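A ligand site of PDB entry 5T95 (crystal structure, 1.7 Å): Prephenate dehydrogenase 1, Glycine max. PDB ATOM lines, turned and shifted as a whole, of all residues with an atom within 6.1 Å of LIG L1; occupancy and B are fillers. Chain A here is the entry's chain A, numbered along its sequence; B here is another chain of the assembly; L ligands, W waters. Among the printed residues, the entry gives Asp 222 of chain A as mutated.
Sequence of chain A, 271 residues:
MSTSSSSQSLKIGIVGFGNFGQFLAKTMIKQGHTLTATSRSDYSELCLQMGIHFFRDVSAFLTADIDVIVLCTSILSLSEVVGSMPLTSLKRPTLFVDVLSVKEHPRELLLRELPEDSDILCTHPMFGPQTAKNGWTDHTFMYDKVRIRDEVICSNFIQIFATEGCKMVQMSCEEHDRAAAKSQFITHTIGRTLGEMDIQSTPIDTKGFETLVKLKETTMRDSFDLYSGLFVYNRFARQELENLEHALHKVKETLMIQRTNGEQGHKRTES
The backbone nitrogen (N) of Pro 129 sits close to an oxygen (O3) of LIG L1 (3.5 Å). N of Phe 127 touches C7 of LIG L1, at 3.9 Å. Hydrophobic or aromatic side chains that line LIG L1: His 124. Of the 20 residues printed, 9 come within 4 Å of LIG L1. The nearest printed residue that does not touch LIG L1 is Leu 226 (4.1 Å).
A nitrogen (N1) of LIG L1 sits close to a nitrogen (N7) of LG2 L2.
OG1 of Thr 131 lies within hydrogen-bond range of N of Gly 128 (3.5 Å). SD of Met 126 sits at hydrogen-bond distance from ND1 of His 124 (3.2 Å). The backbone carbonyl oxygen (O) of Ser 101 sits close to a ring nitrogen (ND1) of His 124, at 3.4 Å.
The side-chain carboxylate (OD2) of Asp 222 lies within salt-bridge range of a nitrogen (N1) of LIG L1 (2.8 Å). An oxygen (O8) of LG2 L2 lies within hydrogen-bond range of the side-chain amide nitrogen of Asn 19. The backbone NH (N) of Thr 131 sits at hydrogen-bond distance from an oxygen (O3) of LIG L1, at 3.1 Å. An oxygen (O3) of LIG L1 lies within hydrogen-bond range of the backbone NH of Gln 130, at 2.9 Å. An oxygen (O13) of LG2 L2 is in hydrogen-bond range of the backbone NH (N) of Ser 101. N of Asn 19 is in hydrogen-bond range of O9 of LG2 L2 (3.3 Å). NE2 of His 124 sits at hydrogen-bond distance from O2 of LIG L1, at 2.5 Å. OG of Ser 101 is in hydrogen-bond range of O13 of LG2 L2 (2.5 Å). The side-chain hydroxyl (OG1) of Thr 131 is in hydrogen-bond range of an oxygen (O1) of LIG L1 (2.5 Å). O3 of LIG L1 sits close to N of Gly 128 (3.2 Å). A nitrogen (N1) of LIG L1 sits at hydrogen-bond distance from the side-chain amide oxygen (OE1) of Gln 130. The side-chain amide nitrogen of Gln 184 lies close to an oxygen (O2) of LIG L1, at 3.1 Å. The side-chain hydroxyl (OG) of Ser 101 sits at hydrogen-bond distance from an oxygen (O2) of LIG L1.
Water W1 lies within hydrogen-bond range of OD2 of Asp 222, O of Thr 218 and N1 of LIG L1.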
ATOM      1  N   ASN A  19      22.430   6.636   1.768  1.00  0.00           N
ATOM      2  CA  ASN A  19      23.885   6.734   1.783  1.00  0.00           C
ATOM      3  C   ASN A  19      24.483   6.738   0.379  1.00  0.00           C
ATOM      4  O   ASN A  19      25.150   7.714  -0.016  1.00  0.00           O
ATOM      5  CB  ASN A  19      24.415   5.567   2.614  1.00  0.00           C
ATOM      6  CG  ASN A  19      25.917   5.487   2.651  1.00  0.00           C
ATOM      7  OD1 ASN A  19      26.610   6.390   3.144  1.00  0.00           O
ATOM      8  ND2 ASN A  19      26.450   4.367   2.165  1.00  0.00           N
ATOM      9  N   VAL A  99      22.341  -0.008  -9.180  1.00  0.00           N
ATOM     10  CA  VAL A  99      23.691   0.038  -8.630  1.00  0.00           C
ATOM     11  C   VAL A  99      23.842  -0.928  -7.462  1.00  0.00           C
ATOM     12  O   VAL A  99      24.747  -0.753  -6.625  1.00  0.00           O
ATOM     13  CB  VAL A  99      24.103   1.466  -8.214  1.00  0.00           C
ATOM     14  CG1 VAL A  99      24.178   2.371  -9.435  1.00  0.00           C
ATOM     15  CG2 VAL A  99      23.169   2.007  -7.127  1.00  0.00           C
ATOM     16  N   LEU A 100      22.989  -1.940  -7.383  1.00  0.00           N
ATOM     17  CA  LEU A 100      23.059  -2.900  -6.286  1.00  0.00           C
ATOM     18  C   LEU A 100      24.394  -3.639  -6.282  1.00  0.00           C
ATOM     19  O   LEU A 100      25.016  -3.851  -7.327  1.00  0.00           O
ATOM     20  CB  LEU A 100      21.906  -3.903  -6.401  1.00  0.00           C
ATOM     21  CG  LEU A 100      20.550  -3.485  -5.808  1.00  0.00           C
ATOM     22  CD1 LEU A 100      19.979  -2.204  -6.417  1.00  0.00           C
ATOM     23  CD2 LEU A 100      19.575  -4.641  -6.036  1.00  0.00           C
ATOM     24  N   SER A 101      24.823  -4.044  -5.090  1.00  0.00           N
ATOM     25  CA  SER A 101      26.108  -4.731  -4.934  1.00  0.00           C
ATOM     26  C   SER A 101      26.068  -6.189  -5.367  1.00  0.00           C
ATOM     27  O   SER A 101      27.118  -6.838  -5.368  1.00  0.00           O
ATOM     28  CB  SER A 101      26.587  -4.648  -3.480  1.00  0.00           C
ATOM     29  OG  SER A 101      26.470  -3.335  -2.961  1.00  0.00           O
ATOM     30  N   HIS A 124      27.625  -2.074 -11.018  1.00  0.00           N
ATOM     31  CA  HIS A 124      28.106  -2.082  -9.632  1.00  0.00           C
ATOM     32  C   HIS A 124      29.346  -1.224  -9.556  1.00  0.00           C
ATOM     33  O   HIS A 124      30.438  -1.650  -9.947  1.00  0.00           O
ATOM     34  CB  HIS A 124      28.399  -3.493  -9.138  1.00  0.00           C
ATOM     35  CG  HIS A 124      28.759  -3.545  -7.686  1.00  0.00           C
ATOM     36  ND1 HIS A 124      29.139  -4.708  -7.050  1.00  0.00           N
ATOM     37  CD2 HIS A 124      28.790  -2.584  -6.732  1.00  0.00           C
ATOM     38  CE1 HIS A 124      29.379  -4.468  -5.772  1.00  0.00           C
ATOM     39  NE2 HIS A 124      29.178  -3.175  -5.555  1.00  0.00           N
ATOM     40  N   PRO A 125      29.231  -0.001  -9.033  1.00  0.00           N
ATOM     41  CA  PRO A 125      30.421   0.747  -8.615  1.00  0.00           C
ATOM     42  C   PRO A 125      31.083   0.012  -7.454  1.00  0.00           C
ATOM     43  O   PRO A 125      30.469  -0.180  -6.396  1.00  0.00           O
ATOM     44  CB  PRO A 125      29.864   2.119  -8.197  1.00  0.00           C
ATOM     45  CG  PRO A 125      28.477   2.177  -8.851  1.00  0.00           C
ATOM     46  CD  PRO A 125      27.987   0.766  -8.819  1.00  0.00           C
ATOM     47  N   MET A 126      32.314  -0.450  -7.654  1.00  0.00           N
ATOM     48  CA  MET A 126      32.965  -1.260  -6.642  1.00  0.00           C
ATOM     49  C   MET A 126      33.634  -0.364  -5.613  1.00  0.00           C
ATOM     50  O   MET A 126      34.798  -0.570  -5.262  1.00  0.00           O
ATOM     51  CB  MET A 126      34.011  -2.201  -7.270  1.00  0.00           C
ATOM     52  CG  MET A 126      33.506  -3.058  -8.421  1.00  0.00           C
ATOM     53  SD  MET A 126      32.087  -4.087  -7.994  1.00  0.00           S
ATOM     54  CE  MET A 126      32.715  -5.133  -6.675  1.00  0.00           C
ATOM     55  N   PHE A 127      32.896   0.641  -5.161  1.00  0.00           N
ATOM     56  CA  PHE A 127      33.450   1.671  -4.281  1.00  0.00           C
ATOM     57  C   PHE A 127      32.295   2.475  -3.728  1.00  0.00           C
ATOM     58  O   PHE A 127      31.153   2.343  -4.170  1.00  0.00           O
ATOM     59  CB  PHE A 127      34.443   2.575  -5.017  1.00  0.00           C
ATOM     60  CG  PHE A 127      33.848   3.287  -6.215  1.00  0.00           C
ATOM     61  CD1 PHE A 127      33.262   4.532  -6.079  1.00  0.00           C
ATOM     62  CD2 PHE A 127      33.897   2.714  -7.489  1.00  0.00           C
ATOM     63  CE1 PHE A 127      32.725   5.204  -7.155  1.00  0.00           C
ATOM     64  CE2 PHE A 127      33.355   3.391  -8.596  1.00  0.00           C
ATOM     65  CZ  PHE A 127      32.766   4.633  -8.418  1.00  0.00           C
ATOM     66  N   GLY A 128      32.611   3.346  -2.768  1.00  0.00           N
ATOM     67  CA  GLY A 128      31.585   4.093  -2.090  1.00  0.00           C
ATOM     68  C   GLY A 128      32.179   5.165  -1.212  1.00  0.00           C
ATOM     69  O   GLY A 128      33.363   5.497  -1.309  1.00  0.00           O
ATOM     70  N   PRO A 129      31.359   5.720  -0.318  1.00  0.00           N
ATOM     71  CA  PRO A 129      31.807   6.882   0.464  1.00  0.00           C
ATOM     72  C   PRO A 129      32.992   6.604   1.376  1.00  0.00           C
ATOM     73  O   PRO A 129      33.630   7.551   1.838  1.00  0.00           O
ATOM     74  CB  PRO A 129      30.561   7.275   1.260  1.00  0.00           C
ATOM     75  CG  PRO A 129      29.572   6.166   1.077  1.00  0.00           C
ATOM     76  CD  PRO A 129      29.915   5.482  -0.200  1.00  0.00           C
ATOM     77  N   GLN A 130      33.322   5.342   1.646  1.00  0.00           N
ATOM     78  CA  GLN A 130      34.488   5.104   2.503  1.00  0.00           C
ATOM     79  C   GLN A 130      35.782   4.988   1.717  1.00  0.00           C
ATOM     80  O   GLN A 130      36.825   5.499   2.142  1.00  0.00           O
ATOM     81  CB  GLN A 130      34.292   3.829   3.331  1.00  0.00           C
ATOM     82  CG  GLN A 130      33.380   4.004   4.535  1.00  0.00           C
ATOM     83  CD  GLN A 130      31.947   4.275   4.150  1.00  0.00           C
ATOM     84  OE1 GLN A 130      31.352   3.533   3.372  1.00  0.00           O
ATOM     85  NE2 GLN A 130      31.388   5.378   4.663  1.00  0.00           N
ATOM     86  N   THR A 131      35.751   4.302   0.574  1.00  0.00           N
ATOM     87  CA  THR A 131      36.960   4.066  -0.181  1.00  0.00           C
ATOM     88  C   THR A 131      37.181   5.086  -1.287  1.00  0.00           C
ATOM     89  O   THR A 131      38.287   5.177  -1.805  1.00  0.00           O
ATOM     90  CB  THR A 131      36.946   2.655  -0.778  1.00  0.00           C
ATOM     91  OG1 THR A 131      35.724   2.445  -1.504  1.00  0.00           O
ATOM     92  CG2 THR A 131      37.059   1.628   0.334  1.00  0.00           C
ATOM     93  N   ALA A 132      36.170   5.875  -1.632  1.00  0.00           N
ATOM     94  CA  ALA A 132      36.293   6.833  -2.724  1.00  0.00           C
ATOM     95  C   ALA A 132      35.818   8.209  -2.298  1.00  0.00           C
ATOM     96  O   ALA A 132      35.163   8.926  -3.059  1.00  0.00           O
ATOM     97  CB  ALA A 132      35.538   6.347  -3.961  1.00  0.00           C
ATOM     98  N   GLN A 184      34.320  -9.435  -2.387  1.00  0.00           N
ATOM     99  CA  GLN A 184      33.596  -8.470  -1.553  1.00  0.00           C
ATOM    100  C   GLN A 184      32.883  -9.155  -0.390  1.00  0.00           C
ATOM    101  O   GLN A 184      32.990  -8.717   0.761  1.00  0.00           O
ATOM    102  CB  GLN A 184      32.614  -7.689  -2.411  1.00  0.00           C
ATOM    103  CG  GLN A 184      31.769  -6.770  -1.582  1.00  0.00           C
ATOM    104  CD  GLN A 184      30.810  -5.994  -2.412  1.00  0.00           C
ATOM    105  OE1 GLN A 184      30.254  -6.502  -3.387  1.00  0.00           O
ATOM    106  NE2 GLN A 184      30.592  -4.749  -2.041  1.00  0.00           N
ATOM    107  N   HIS A 188      33.617  -8.408   3.487  1.00  0.00           N
ATOM    108  CA  HIS A 188      32.709  -7.760   4.409  1.00  0.00           C
ATOM    109  C   HIS A 188      32.340  -8.698   5.554  1.00  0.00           C
ATOM    110  O   HIS A 188      32.077  -8.240   6.662  1.00  0.00           O
ATOM    111  CB  HIS A 188      31.464  -7.224   3.668  1.00  0.00           C
ATOM    112  CG  HIS A 188      30.750  -6.187   4.439  1.00  0.00           C
ATOM    113  ND1 HIS A 188      30.298  -6.380   5.710  1.00  0.00           N
ATOM    114  CD2 HIS A 188      30.421  -4.915   4.105  1.00  0.00           C
ATOM    115  CE1 HIS A 188      29.597  -5.304   6.083  1.00  0.00           C
ATOM    116  NE2 HIS A 188      29.756  -4.357   5.171  1.00  0.00           N
ATOM    117  N   THR A 218      35.658   0.706   8.473  1.00  0.00           N
ATOM    118  CA  THR A 218      34.997   0.967   7.194  1.00  0.00           C
ATOM    119  C   THR A 218      33.792   0.062   7.008  1.00  0.00           C
ATOM    120  O   THR A 218      32.729   0.497   6.545  1.00  0.00           O
ATOM    121  CB  THR A 218      36.000   0.756   6.064  1.00  0.00           C
ATOM    122  OG1 THR A 218      36.944   1.834   6.064  1.00  0.00           O
ATOM    123  CG2 THR A 218      35.304   0.670   4.713  1.00  0.00           C
ATOM    124  N   ASP A 222      28.612   0.504   6.794  1.00  0.00           N
ATOM    125  CA  ASP A 222      27.527   0.045   5.936  1.00  0.00           C
ATOM    126  C   ASP A 222      26.442  -0.635   6.761  1.00  0.00           C
ATOM    127  O   ASP A 222      26.688  -1.132   7.861  1.00  0.00           O
ATOM    128  CB  ASP A 222      28.055  -0.933   4.865  1.00  0.00           C
ATOM    129  CG  ASP A 222      28.776  -0.219   3.758  1.00  0.00           C
ATOM    130  OD1 ASP A 222      28.253   0.816   3.316  1.00  0.00           O
ATOM    131  OD2 ASP A 222      29.878  -0.655   3.368  1.00  0.00           O
ATOM    132  N   LEU A 226      22.611  -4.072   3.908  1.00  0.00           N
ATOM    133  CA  LEU A 226      23.513  -4.236   2.775  1.00  0.00           C
ATOM    134  C   LEU A 226      24.267  -5.557   2.894  1.00  0.00           C
ATOM    135  O   LEU A 226      24.333  -6.323   1.935  1.00  0.00           O
ATOM    136  CB  LEU A 226      24.485  -3.047   2.702  1.00  0.00           C
ATOM    137  CG  LEU A 226      25.421  -3.001   1.479  1.00  0.00           C
ATOM    138  CD1 LEU A 226      25.721  -1.559   1.111  1.00  0.00           C
ATOM    139  CD2 LEU A 226      26.713  -3.793   1.743  1.00  0.00           C
ATOM    140  N   LEU A 230      24.173  -9.003   0.387  1.00  0.00           N
ATOM    141  CA  LEU A 230      25.297  -9.635  -0.292  1.00  0.00           C
ATOM    142  C   LEU A 230      25.220 -11.134  -0.212  1.00  0.00           C
ATOM    143  O   LEU A 230      25.718 -11.824  -1.111  1.00  0.00           O
ATOM    144  CB  LEU A 230      26.639  -9.187   0.306  1.00  0.00           C
ATOM    145  CG  LEU A 230      26.895  -7.682   0.415  1.00  0.00           C
ATOM    146  CD1 LEU A 230      28.320  -7.475   0.939  1.00  0.00           C
ATOM    147  CD2 LEU A 230      26.695  -6.975  -0.909  1.00  0.00           C
ATOM    148  N   THR B 206      37.320  -4.902  -4.678  1.00  0.00           N
ATOM    149  CA  THR B 206      37.194  -3.687  -3.876  1.00  0.00           C
ATOM    150  C   THR B 206      38.546  -3.402  -3.222  1.00  0.00           C
ATOM    151  O   THR B 206      39.412  -4.266  -3.121  1.00  0.00           O
ATOM    152  CB  THR B 206      36.105  -3.835  -2.820  1.00  0.00           C
ATOM    153  OG1 THR B 206      36.437  -4.932  -1.952  1.00  0.00           O
ATOM    154  CG2 THR B 206      34.742  -4.100  -3.475  1.00  0.00           C
HETATM  155  N1  LIG L   1      31.108   1.226   1.632  1.00  0.00           N
HETATM  156  C1  LIG L   1      32.458   0.715   1.413  1.00  0.00           C
HETATM  157  C2  LIG L   1      33.230   1.536   0.395  1.00  0.00           C
HETATM  158  O1  LIG L   1      34.050   1.002  -0.360  1.00  0.00           O
HETATM  159  C3  LIG L   1      32.412  -0.759   1.004  1.00  0.00           C
HETATM  160  C4  LIG L   1      31.459  -1.164  -0.126  1.00  0.00           C
HETATM  161  C5  LIG L   1      31.854  -1.125  -1.456  1.00  0.00           C
HETATM  162  C6  LIG L   1      30.193  -1.664   0.153  1.00  0.00           C
HETATM  163  C7  LIG L   1      31.008  -1.540  -2.477  1.00  0.00           C
HETATM  164  C8  LIG L   1      29.337  -2.077  -0.857  1.00  0.00           C
HETATM  165  C9  LIG L   1      29.756  -2.013  -2.163  1.00  0.00           C
HETATM  166  O2  LIG L   1      28.913  -2.435  -3.163  1.00  0.00           O
HETATM  167  O3  LIG L   1      33.048   2.751   0.305  1.00  0.00           O
HETATM  168  P1  LG2 L   2      21.426   0.303   1.861  1.00  0.00           P
HETATM  169  O1  LG2 L   2      21.114   0.067   3.334  1.00  0.00           O
HETATM  170  O2  LG2 L   2      21.737  -0.992   1.148  1.00  0.00           O
HETATM  171  O3  LG2 L   2      20.154   0.965   1.155  1.00  0.00           O
HETATM  172  C1  LG2 L   2      19.690   2.221   1.651  1.00  0.00           C
HETATM  173  C2  LG2 L   2      18.518   2.616   0.698  1.00  0.00           C
HETATM  174  O4  LG2 L   2      17.636   1.643   0.713  1.00  0.00           O
HETATM  175  C3  LG2 L   2      17.829   3.869   1.235  1.00  0.00           C
HETATM  176  O5  LG2 L   2      17.684   4.803   0.245  1.00  0.00           O
HETATM  177  C4  LG2 L   2      16.501   3.319   1.787  1.00  0.00           C
HETATM  178  O6  LG2 L   2      15.408   4.334   1.735  1.00  0.00           O
HETATM  179  C5  LG2 L   2      16.218   2.340   0.973  1.00  0.00           C
HETATM  180  N1  LG2 L   2      15.430   1.321   1.576  1.00  0.00           N
HETATM  181  C6  LG2 L   2      15.816   0.405   2.488  1.00  0.00           C
HETATM  182  N2  LG2 L   2      14.748  -0.368   2.784  1.00  0.00           N
HETATM  183  C7  LG2 L   2      13.696   0.084   2.040  1.00  0.00           C
HETATM  184  C8  LG2 L   2      12.379  -0.341   1.966  1.00  0.00           C
HETATM  185  N3  LG2 L   2      11.568  -1.363   2.553  1.00  0.00           N
HETATM  186  N4  LG2 L   2      11.515   0.278   1.149  1.00  0.00           N
HETATM  187  C9  LG2 L   2      11.927   1.329   0.389  1.00  0.00           C
HETATM  188  N5  LG2 L   2      13.234   1.754   0.464  1.00  0.00           N
HETATM  189  C10 LG2 L   2      14.099   1.126   1.293  1.00  0.00           C
HETATM  190  O7  LG2 L   2      22.646   1.324   1.883  1.00  0.00           O
HETATM  191  P2  LG2 L   2      23.334   2.167   0.698  1.00  0.00           P
HETATM  192  O8  LG2 L   2      24.783   2.243   1.096  1.00  0.00           O
HETATM  193  O9  LG2 L   2      22.680   3.522   0.581  1.00  0.00           O
HETATM  194  O10 LG2 L   2      23.245   1.325  -0.646  1.00  0.00           O
HETATM  195  C11 LG2 L   2      22.203   1.569  -1.552  1.00  0.00           C
HETATM  196  C12 LG2 L   2      22.467   0.637  -2.777  1.00  0.00           C
HETATM  197  O11 LG2 L   2      23.651   0.914  -3.295  1.00  0.00           O
HETATM  198  C13 LG2 L   2      22.501  -0.821  -2.331  1.00  0.00           C
HETATM  199  O12 LG2 L   2      21.858  -1.636  -3.244  1.00  0.00           O
HETATM  200  C14 LG2 L   2      24.004  -1.106  -2.311  1.00  0.00           C
HETATM  201  O13 LG2 L   2      24.135  -2.594  -2.396  1.00  0.00           O
HETATM  202  C15 LG2 L   2      24.493  -0.440  -3.347  1.00  0.00           C
HETATM  203  N6  LG2 L   2      25.840  -0.014  -3.206  1.00  0.00           N
HETATM  204  C16 LG2 L   2      26.282   0.542  -2.029  1.00  0.00           C
HETATM  205  C17 LG2 L   2      27.601   0.969  -1.946  1.00  0.00           C
HETATM  206  C18 LG2 L   2      28.128   1.584  -0.667  1.00  0.00           C
HETATM  207  O14 LG2 L   2      27.426   1.814   0.315  1.00  0.00           O
HETATM  208  N7  LG2 L   2      29.521   1.873  -0.643  1.00  0.00           N
HETATM  209  C19 LG2 L   2      28.452   0.844  -3.006  1.00  0.00           C
HETATM  210  C20 LG2 L   2      28.000   0.300  -4.174  1.00  0.00           C
HETATM  211  C21 LG2 L   2      26.680  -0.128  -4.267  1.00  0.00           C
HETATM  212  P3  LG2 L   2      15.347   5.589   2.716  1.00  0.00           P
HETATM  213  O15 LG2 L   2      16.754   6.172   2.864  1.00  0.00           O
HETATM  214  O16 LG2 L   2      14.460   6.607   2.051  1.00  0.00           O
HETATM  215  O17 LG2 L   2      14.766   5.129   4.048  1.00  0.00           O
HETATM  216  O   HOH W   1      32.309  -0.740   4.247  1.00  0.00           O
HETATM  217  O   HOH W   2      28.809   3.370   2.804  1.00  0.00           O
